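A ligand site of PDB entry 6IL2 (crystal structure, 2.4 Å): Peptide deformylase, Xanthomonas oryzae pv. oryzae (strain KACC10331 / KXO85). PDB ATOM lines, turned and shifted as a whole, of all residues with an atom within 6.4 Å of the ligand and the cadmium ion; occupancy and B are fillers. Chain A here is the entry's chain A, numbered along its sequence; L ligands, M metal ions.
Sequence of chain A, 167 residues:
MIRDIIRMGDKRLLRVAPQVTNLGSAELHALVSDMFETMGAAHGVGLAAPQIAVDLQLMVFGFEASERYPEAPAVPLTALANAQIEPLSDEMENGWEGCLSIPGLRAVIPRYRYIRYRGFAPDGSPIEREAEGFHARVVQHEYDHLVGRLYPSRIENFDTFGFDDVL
Gly 44 touches the ligand.
Gly 46 touches the ligand (O to C10, 3.5 Å).
Trp 96 touches the ligand.
Glu 97 touches the ligand (CG to C9, 3.7 Å).
O of Gly 98 touches C1 of the ligand, at 3.6 Å.
CE1 of Phe 134 touches C9 of the ligand, at 3.8 Å.
CG of Arg 137 touches C7 of the ligand, at 3.95 Å.
Hydrophobic or aromatic side chains that line the ligand: Val 45, Leu 100, Phe 134, His 141 and His 145.
Within 4 Å of the ligand: Gly 44, Val 45, Gly 46, Gln 51, Trp 96, Glu 97, Gly 98, CSD 99, Leu 100, Phe 134, Arg 137, His 141, Glu 142 and His 145.
Gln 51 touches the cadmium ion (NE2 to CD, 3.5 Å).
Four residues have an atom within 4 Å of the cadmium ion: Gln 51, CSD 99, His 141 and His 145.
The cadmium ion is bound by an oxygen (O4) of the ligand (1.9 Å), a ring nitrogen (NE2) of His 145 (2.3 Å), a ring nitrogen (NE2) of His 141 (2.4 Å) and SG of CSD 99 (2.6 Å).
Slightly farther from the cadmium ion lies O3 of the ligand (2.8 Å).
N2 of the ligand sits close to OE2 of Glu 142 (2.5 Å).
NE2 of Gln 51 is in hydrogen-bond range of O3 of the ligand.
The backbone NH of Val 45 lies within hydrogen-bond range of an oxygen (O2) of the ligand (3.0 Å).
O3 of the ligand sits at hydrogen-bond distance from N of Leu 100 (3.0 Å).
OE1 of Glu 97 lies within hydrogen-bond range of ND1 of His 141 (2.7 Å).
The side-chain carboxylate (OE1) of Glu 142 sits close to the side-chain amide oxygen (OE1) of Gln 51 (3.5 Å).
N of Ala 48 is in hydrogen-bond range of OE1 of Glu 142, at 3.2 Å.
The side-chain amide nitrogen (NE2) of Gln 51 is in hydrogen-bond range of OD1 of CSD 99.
OD1 of CSD 99 sits at hydrogen-bond distance from the backbone NH of Ser 101 (2.9 Å).
The side-chain hydroxyl of Ser 101 sits at hydrogen-bond distance from the side-chain amide nitrogen of Gln 51.
NH1 of Arg 137 lies within salt-bridge range of OE2 of Glu 97 (2.9 Å).
The guanidinium group (NE) of Arg 111 is in salt-bridge range of the side-chain carboxylate (OE2) of Glu 97.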
ATOM      1  N   HIS A  43     -16.254 -19.085  13.814  1.00  0.00           N
ATOM      2  CA  HIS A  43     -15.246 -18.585  14.798  1.00  0.00           C
ATOM      3  C   HIS A  43     -15.755 -17.517  15.744  1.00  0.00           C
ATOM      4  O   HIS A  43     -14.972 -16.714  16.257  1.00  0.00           O
ATOM      5  CB  HIS A  43     -13.938 -18.105  14.150  1.00  0.00           C
ATOM      6  CG  HIS A  43     -13.156 -19.197  13.487  1.00  0.00           C
ATOM      7  ND1 HIS A  43     -11.797 -19.298  13.613  1.00  0.00           N
ATOM      8  CD2 HIS A  43     -13.534 -20.231  12.698  1.00  0.00           C
ATOM      9  CE1 HIS A  43     -11.361 -20.343  12.926  1.00  0.00           C
ATOM     10  NE2 HIS A  43     -12.402 -20.925  12.366  1.00  0.00           N
ATOM     11  N   GLY A  44     -17.060 -17.546  16.057  1.00  0.00           N
ATOM     12  CA  GLY A  44     -17.630 -16.591  16.990  1.00  0.00           C
ATOM     13  C   GLY A  44     -17.562 -17.011  18.412  1.00  0.00           C
ATOM     14  O   GLY A  44     -17.273 -18.155  18.693  1.00  0.00           O
ATOM     15  N   VAL A  45     -17.832 -16.075  19.322  1.00  0.00           N
ATOM     16  CA  VAL A  45     -18.103 -16.413  20.700  1.00  0.00           C
ATOM     17  C   VAL A  45     -19.588 -16.301  21.061  1.00  0.00           C
ATOM     18  O   VAL A  45     -19.978 -16.525  22.209  1.00  0.00           O
ATOM     19  CB  VAL A  45     -17.244 -15.596  21.651  1.00  0.00           C
ATOM     20  CG1 VAL A  45     -15.771 -15.874  21.341  1.00  0.00           C
ATOM     21  CG2 VAL A  45     -17.593 -14.112  21.605  1.00  0.00           C
ATOM     22  N   GLY A  46     -20.435 -15.993  20.090  1.00  0.00           N
ATOM     23  CA  GLY A  46     -21.815 -15.727  20.395  1.00  0.00           C
ATOM     24  C   GLY A  46     -22.515 -15.830  19.063  1.00  0.00           C
ATOM     25  O   GLY A  46     -21.852 -15.672  18.010  1.00  0.00           O
ATOM     26  N   LEU A  47     -23.794 -16.184  19.097  1.00  0.00           N
ATOM     27  CA  LEU A  47     -24.595 -16.234  17.886  1.00  0.00           C
ATOM     28  C   LEU A  47     -26.053 -16.175  18.309  1.00  0.00           C
ATOM     29  O   LEU A  47     -26.456 -16.920  19.146  1.00  0.00           O
ATOM     30  CB  LEU A  47     -24.321 -17.506  17.131  1.00  0.00           C
ATOM     31  CG  LEU A  47     -25.058 -17.613  15.779  1.00  0.00           C
ATOM     32  CD1 LEU A  47     -24.291 -16.840  14.723  1.00  0.00           C
ATOM     33  CD2 LEU A  47     -25.296 -19.053  15.321  1.00  0.00           C
ATOM     34  N   ALA A  48     -26.819 -15.251  17.754  1.00  0.00           N
ATOM     35  CA  ALA A  48     -28.226 -15.190  18.061  1.00  0.00           C
ATOM     36  C   ALA A  48     -28.994 -15.748  16.906  1.00  0.00           C
ATOM     37  O   ALA A  48     -28.575 -15.706  15.770  1.00  0.00           O
ATOM     38  CB  ALA A  48     -28.629 -13.783  18.335  1.00  0.00           C
ATOM     39  N   GLN A  51     -29.540 -14.058  13.587  1.00  0.00           N
ATOM     40  CA  GLN A  51     -28.408 -14.099  12.685  1.00  0.00           C
ATOM     41  C   GLN A  51     -28.489 -15.218  11.678  1.00  0.00           C
ATOM     42  O   GLN A  51     -27.909 -15.094  10.642  1.00  0.00           O
ATOM     43  CB  GLN A  51     -27.067 -14.113  13.402  1.00  0.00           C
ATOM     44  CG  GLN A  51     -26.840 -12.906  14.256  1.00  0.00           C
ATOM     45  CD  GLN A  51     -25.436 -12.860  14.830  1.00  0.00           C
ATOM     46  OE1 GLN A  51     -25.214 -13.318  15.931  1.00  0.00           O
ATOM     47  NE2 GLN A  51     -24.477 -12.382  14.047  1.00  0.00           N
ATOM     48  N   TRP A  96     -13.843  -3.783  22.802  1.00  0.00           N
ATOM     49  CA  TRP A  96     -14.013  -4.152  21.401  1.00  0.00           C
ATOM     50  C   TRP A  96     -15.161  -5.095  21.086  1.00  0.00           C
ATOM     51  O   TRP A  96     -15.392  -6.088  21.792  1.00  0.00           O
ATOM     52  CB  TRP A  96     -12.722  -4.774  20.929  1.00  0.00           C
ATOM     53  CG  TRP A  96     -11.625  -3.714  20.873  1.00  0.00           C
ATOM     54  CD1 TRP A  96     -10.580  -3.556  21.726  1.00  0.00           C
ATOM     55  CD2 TRP A  96     -11.507  -2.648  19.888  1.00  0.00           C
ATOM     56  NE1 TRP A  96      -9.808  -2.462  21.340  1.00  0.00           N
ATOM     57  CE2 TRP A  96     -10.346  -1.906  20.211  1.00  0.00           C
ATOM     58  CE3 TRP A  96     -12.272  -2.258  18.795  1.00  0.00           C
ATOM     59  CZ2 TRP A  96      -9.937  -0.797  19.461  1.00  0.00           C
ATOM     60  CZ3 TRP A  96     -11.856  -1.177  18.048  1.00  0.00           C
ATOM     61  CH2 TRP A  96     -10.695  -0.448  18.386  1.00  0.00           C
ATOM     62  N   GLU A  97     -15.873  -4.852  19.999  1.00  0.00           N
ATOM     63  CA  GLU A  97     -16.823  -5.881  19.499  1.00  0.00           C
ATOM     64  C   GLU A  97     -16.723  -6.049  18.002  1.00  0.00           C
ATOM     65  O   GLU A  97     -16.179  -5.184  17.324  1.00  0.00           O
ATOM     66  CB  GLU A  97     -18.266  -5.488  19.847  1.00  0.00           C
ATOM     67  CG  GLU A  97     -18.462  -5.283  21.370  1.00  0.00           C
ATOM     68  CD  GLU A  97     -19.933  -5.153  21.803  1.00  0.00           C
ATOM     69  OE1 GLU A  97     -20.844  -5.376  20.968  1.00  0.00           O
ATOM     70  OE2 GLU A  97     -20.197  -4.818  22.993  1.00  0.00           O
ATOM     71  N   GLY A  98     -17.210  -7.189  17.528  1.00  0.00           N
ATOM     72  CA  GLY A  98     -17.521  -7.448  16.123  1.00  0.00           C
ATOM     73  C   GLY A  98     -18.854  -8.180  15.973  1.00  0.00           C
ATOM     74  O   GLY A  98     -19.627  -8.320  16.912  1.00  0.00           O
ATOM     75  N   CSD A  99     -19.119  -8.654  14.781  1.00  0.00           N
ATOM     76  CA  CSD A  99     -20.432  -9.172  14.447  1.00  0.00           C
ATOM     77  CB  CSD A  99     -21.467  -8.066  14.200  1.00  0.00           C
ATOM     78  SG  CSD A  99     -23.087  -8.427  14.664  1.00  0.00           S
ATOM     79  C   CSD A  99     -20.176 -10.048  13.239  1.00  0.00           C
ATOM     80  O   CSD A  99     -19.572  -9.619  12.252  1.00  0.00           O
ATOM     81  OD1 CSD A  99     -23.283  -9.512  13.707  1.00  0.00           O
ATOM     82  OD2 CSD A  99     -23.853  -7.449  13.577  1.00  0.00           O
ATOM     83  N   LEU A 100     -20.610 -11.296  13.347  1.00  0.00           N
ATOM     84  CA  LEU A 100     -20.488 -12.217  12.250  1.00  0.00           C
ATOM     85  C   LEU A 100     -21.362 -11.729  11.103  1.00  0.00           C
ATOM     86  O   LEU A 100     -21.124 -12.110   9.964  1.00  0.00           O
ATOM     87  CB  LEU A 100     -20.900 -13.633  12.667  1.00  0.00           C
ATOM     88  CG  LEU A 100     -20.022 -14.191  13.765  1.00  0.00           C
ATOM     89  CD1 LEU A 100     -20.655 -15.464  14.350  1.00  0.00           C
ATOM     90  CD2 LEU A 100     -18.608 -14.391  13.238  1.00  0.00           C
ATOM     91  N   SER A 101     -22.355 -10.908  11.399  1.00  0.00           N
ATOM     92  CA  SER A 101     -23.171 -10.277  10.345  1.00  0.00           C
ATOM     93  C   SER A 101     -22.547  -9.001   9.749  1.00  0.00           C
ATOM     94  O   SER A 101     -23.076  -8.493   8.765  1.00  0.00           O
ATOM     95  CB  SER A 101     -24.617 -10.019  10.882  1.00  0.00           C
ATOM     96  OG  SER A 101     -25.246 -11.270  11.244  1.00  0.00           O
ATOM     97  N   ARG A 111     -20.754  -0.998  27.309  1.00  0.00           N
ATOM     98  CA  ARG A 111     -21.752  -1.901  27.838  1.00  0.00           C
ATOM     99  C   ARG A 111     -21.697  -1.837  29.360  1.00  0.00           C
ATOM    100  O   ARG A 111     -20.686  -1.424  29.927  1.00  0.00           O
ATOM    101  CB  ARG A 111     -21.422  -3.346  27.457  1.00  0.00           C
ATOM    102  CG  ARG A 111     -21.296  -3.653  25.971  1.00  0.00           C
ATOM    103  CD  ARG A 111     -22.681  -3.687  25.329  1.00  0.00           C
ATOM    104  NE  ARG A 111     -22.587  -4.123  23.953  1.00  0.00           N
ATOM    105  CZ  ARG A 111     -23.614  -4.218  23.091  1.00  0.00           C
ATOM    106  NH1 ARG A 111     -24.854  -3.925  23.444  1.00  0.00           N
ATOM    107  NH2 ARG A 111     -23.371  -4.611  21.819  1.00  0.00           N
ATOM    108  N   PHE A 134     -16.387  -9.380  30.063  1.00  0.00           N
ATOM    109  CA  PHE A 134     -16.538 -10.038  28.793  1.00  0.00           C
ATOM    110  C   PHE A 134     -17.771 -10.948  28.665  1.00  0.00           C
ATOM    111  O   PHE A 134     -18.466 -10.850  27.690  1.00  0.00           O
ATOM    112  CB  PHE A 134     -15.273 -10.776  28.336  1.00  0.00           C
ATOM    113  CG  PHE A 134     -15.312 -11.075  26.845  1.00  0.00           C
ATOM    114  CD1 PHE A 134     -15.422 -10.055  25.924  1.00  0.00           C
ATOM    115  CD2 PHE A 134     -15.267 -12.371  26.364  1.00  0.00           C
ATOM    116  CE1 PHE A 134     -15.479 -10.324  24.555  1.00  0.00           C
ATOM    117  CE2 PHE A 134     -15.337 -12.642  25.004  1.00  0.00           C
ATOM    118  CZ  PHE A 134     -15.453 -11.628  24.104  1.00  0.00           C
ATOM    119  N   ARG A 137     -20.711  -8.756  28.388  1.00  0.00           N
ATOM    120  CA  ARG A 137     -20.736  -8.063  27.082  1.00  0.00           C
ATOM    121  C   ARG A 137     -21.323  -8.927  25.987  1.00  0.00           C
ATOM    122  O   ARG A 137     -22.180  -8.460  25.227  1.00  0.00           O
ATOM    123  CB  ARG A 137     -19.303  -7.616  26.710  1.00  0.00           C
ATOM    124  CG  ARG A 137     -19.118  -7.076  25.307  1.00  0.00           C
ATOM    125  CD  ARG A 137     -17.719  -6.559  25.132  1.00  0.00           C
ATOM    126  NE  ARG A 137     -17.408  -5.502  26.099  1.00  0.00           N
ATOM    127  CZ  ARG A 137     -17.661  -4.198  25.925  1.00  0.00           C
ATOM    128  NH1 ARG A 137     -18.224  -3.750  24.804  1.00  0.00           N
ATOM    129  NH2 ARG A 137     -17.337  -3.351  26.878  1.00  0.00           N
ATOM    130  N   VAL A 138     -20.848 -10.163  25.900  1.00  0.00           N
ATOM    131  CA  VAL A 138     -21.334 -11.102  24.893  1.00  0.00           C
ATOM    132  C   VAL A 138     -22.832 -11.298  25.014  1.00  0.00           C
ATOM    133  O   VAL A 138     -23.545 -11.276  23.997  1.00  0.00           O
ATOM    134  CB  VAL A 138     -20.629 -12.432  24.954  1.00  0.00           C
ATOM    135  CG1 VAL A 138     -21.212 -13.350  23.891  1.00  0.00           C
ATOM    136  CG2 VAL A 138     -19.140 -12.264  24.658  1.00  0.00           C
ATOM    137  N   VAL A 139     -23.319 -11.339  26.253  1.00  0.00           N
ATOM    138  CA  VAL A 139     -24.730 -11.495  26.471  1.00  0.00           C
ATOM    139  C   VAL A 139     -25.541 -10.272  26.076  1.00  0.00           C
ATOM    140  O   VAL A 139     -26.637 -10.402  25.475  1.00  0.00           O
ATOM    141  CB  VAL A 139     -25.017 -11.932  27.920  1.00  0.00           C
ATOM    142  CG1 VAL A 139     -26.509 -12.083  28.177  1.00  0.00           C
ATOM    143  CG2 VAL A 139     -24.340 -13.305  28.196  1.00  0.00           C
ATOM    144  N   HIS A 141     -24.726  -8.070  23.886  1.00  0.00           N
ATOM    145  CA  HIS A 141     -24.585  -8.017  22.430  1.00  0.00           C
ATOM    146  C   HIS A 141     -25.613  -8.959  21.760  1.00  0.00           C
ATOM    147  O   HIS A 141     -26.241  -8.589  20.834  1.00  0.00           O
ATOM    148  CB  HIS A 141     -23.150  -8.410  22.041  1.00  0.00           C
ATOM    149  CG  HIS A 141     -22.908  -8.457  20.569  1.00  0.00           C
ATOM    150  ND1 HIS A 141     -22.273  -7.438  19.876  1.00  0.00           N
ATOM    151  CD2 HIS A 141     -23.190  -9.413  19.655  1.00  0.00           C
ATOM    152  CE1 HIS A 141     -22.221  -7.758  18.589  1.00  0.00           C
ATOM    153  NE2 HIS A 141     -22.748  -8.961  18.447  1.00  0.00           N
ATOM    154  N   GLU A 142     -25.735 -10.191  22.229  1.00  0.00           N
ATOM    155  CA  GLU A 142     -26.658 -11.094  21.602  1.00  0.00           C
ATOM    156  C   GLU A 142     -28.066 -10.716  21.926  1.00  0.00           C
ATOM    157  O   GLU A 142     -28.952 -10.837  21.090  1.00  0.00           O
ATOM    158  CB  GLU A 142     -26.439 -12.515  22.073  1.00  0.00           C
ATOM    159  CG  GLU A 142     -25.103 -13.172  21.721  1.00  0.00           C
ATOM    160  CD  GLU A 142     -24.597 -12.886  20.313  1.00  0.00           C
ATOM    161  OE1 GLU A 142     -25.441 -12.863  19.355  1.00  0.00           O
ATOM    162  OE2 GLU A 142     -23.349 -12.734  20.188  1.00  0.00           O
ATOM    163  N   HIS A 145     -29.388  -8.416  19.415  1.00  0.00           N
ATOM    164  CA  HIS A 145     -29.975  -9.090  18.250  1.00  0.00           C
ATOM    165  C   HIS A 145     -31.431  -9.455  18.395  1.00  0.00           C
ATOM    166  O   HIS A 145     -32.179  -9.408  17.426  1.00  0.00           O
ATOM    167  CB  HIS A 145     -29.235 -10.361  17.865  1.00  0.00           C
ATOM    168  CG  HIS A 145     -27.959 -10.099  17.180  1.00  0.00           C
ATOM    169  ND1 HIS A 145     -27.888  -9.426  15.998  1.00  0.00           N
ATOM    170  CD2 HIS A 145     -26.697 -10.410  17.516  1.00  0.00           C
ATOM    171  CE1 HIS A 145     -26.634  -9.369  15.585  1.00  0.00           C
ATOM    172  NE2 HIS A 145     -25.894  -9.953  16.500  1.00  0.00           N
ATOM    173  N   LEU A 150     -28.189  -3.560  16.361  1.00  0.00           N
ATOM    174  CA  LEU A 150     -26.798  -3.920  16.039  1.00  0.00           C
ATOM    175  C   LEU A 150     -25.790  -2.946  16.642  1.00  0.00           C
ATOM    176  O   LEU A 150     -26.126  -1.760  16.883  1.00  0.00           O
ATOM    177  CB  LEU A 150     -26.635  -3.875  14.524  1.00  0.00           C
ATOM    178  CG  LEU A 150     -27.655  -4.730  13.757  1.00  0.00           C
ATOM    179  CD1 LEU A 150     -27.619  -4.436  12.269  1.00  0.00           C
ATOM    180  CD2 LEU A 150     -27.404  -6.226  14.068  1.00  0.00           C
ATOM    181  N   TYR A 151     -24.552  -3.390  16.814  1.00  0.00           N
ATOM    182  CA  TYR A 151     -23.549  -2.550  17.485  1.00  0.00           C
ATOM    183  C   TYR A 151     -23.248  -1.142  16.918  1.00  0.00           C
ATOM    184  O   TYR A 151     -22.979  -0.261  17.708  1.00  0.00           O
ATOM    185  CB  TYR A 151     -22.262  -3.299  17.776  1.00  0.00           C
ATOM    186  CG  TYR A 151     -21.271  -3.412  16.676  1.00  0.00           C
ATOM    187  CD1 TYR A 151     -20.469  -2.326  16.271  1.00  0.00           C
ATOM    188  CD2 TYR A 151     -21.062  -4.620  16.055  1.00  0.00           C
ATOM    189  CE1 TYR A 151     -19.513  -2.475  15.272  1.00  0.00           C
ATOM    190  CE2 TYR A 151     -20.142  -4.773  15.036  1.00  0.00           C
ATOM    191  CZ  TYR A 151     -19.373  -3.708  14.650  1.00  0.00           C
ATOM    192  OH  TYR A 151     -18.500  -3.962  13.631  1.00  0.00           O
HETATM  193  N1  LIG L   1     -20.510 -12.412  17.086  1.00  0.00           N
HETATM  194  C1  LIG L   1     -19.616 -11.757  18.014  1.00  0.00           C
HETATM  195  C2  LIG L   1     -18.300 -12.348  17.505  1.00  0.00           C
HETATM  196  O1  LIG L   1     -17.439 -11.740  16.604  1.00  0.00           O
HETATM  197  C3  LIG L   1     -19.904 -11.858  19.525  1.00  0.00           C
HETATM  198  C4  LIG L   1     -19.104 -10.818  20.294  1.00  0.00           C
HETATM  199  C5  LIG L   1     -19.808  -9.946  21.116  1.00  0.00           C
HETATM  200  C6  LIG L   1     -17.698 -10.716  20.203  1.00  0.00           C
HETATM  201  C7  LIG L   1     -19.112  -8.996  21.851  1.00  0.00           C
HETATM  202  C8  LIG L   1     -16.989  -9.777  20.942  1.00  0.00           C
HETATM  203  C9  LIG L   1     -17.708  -8.915  21.781  1.00  0.00           C
HETATM  204  O2  LIG L   1     -18.133 -13.482  17.908  1.00  0.00           O
HETATM  205  C10 LIG L   1     -21.805 -12.299  16.922  1.00  0.00           C
HETATM  206  O3  LIG L   1     -22.117 -12.278  15.729  1.00  0.00           O
HETATM  207  N2  LIG L   1     -22.690 -12.038  17.906  1.00  0.00           N
HETATM  208  O4  LIG L   1     -23.982 -11.705  17.575  1.00  0.00           O
HETATM  209 CD    CD M   1     -23.595 -10.096  16.548  1.00  0.00          CD
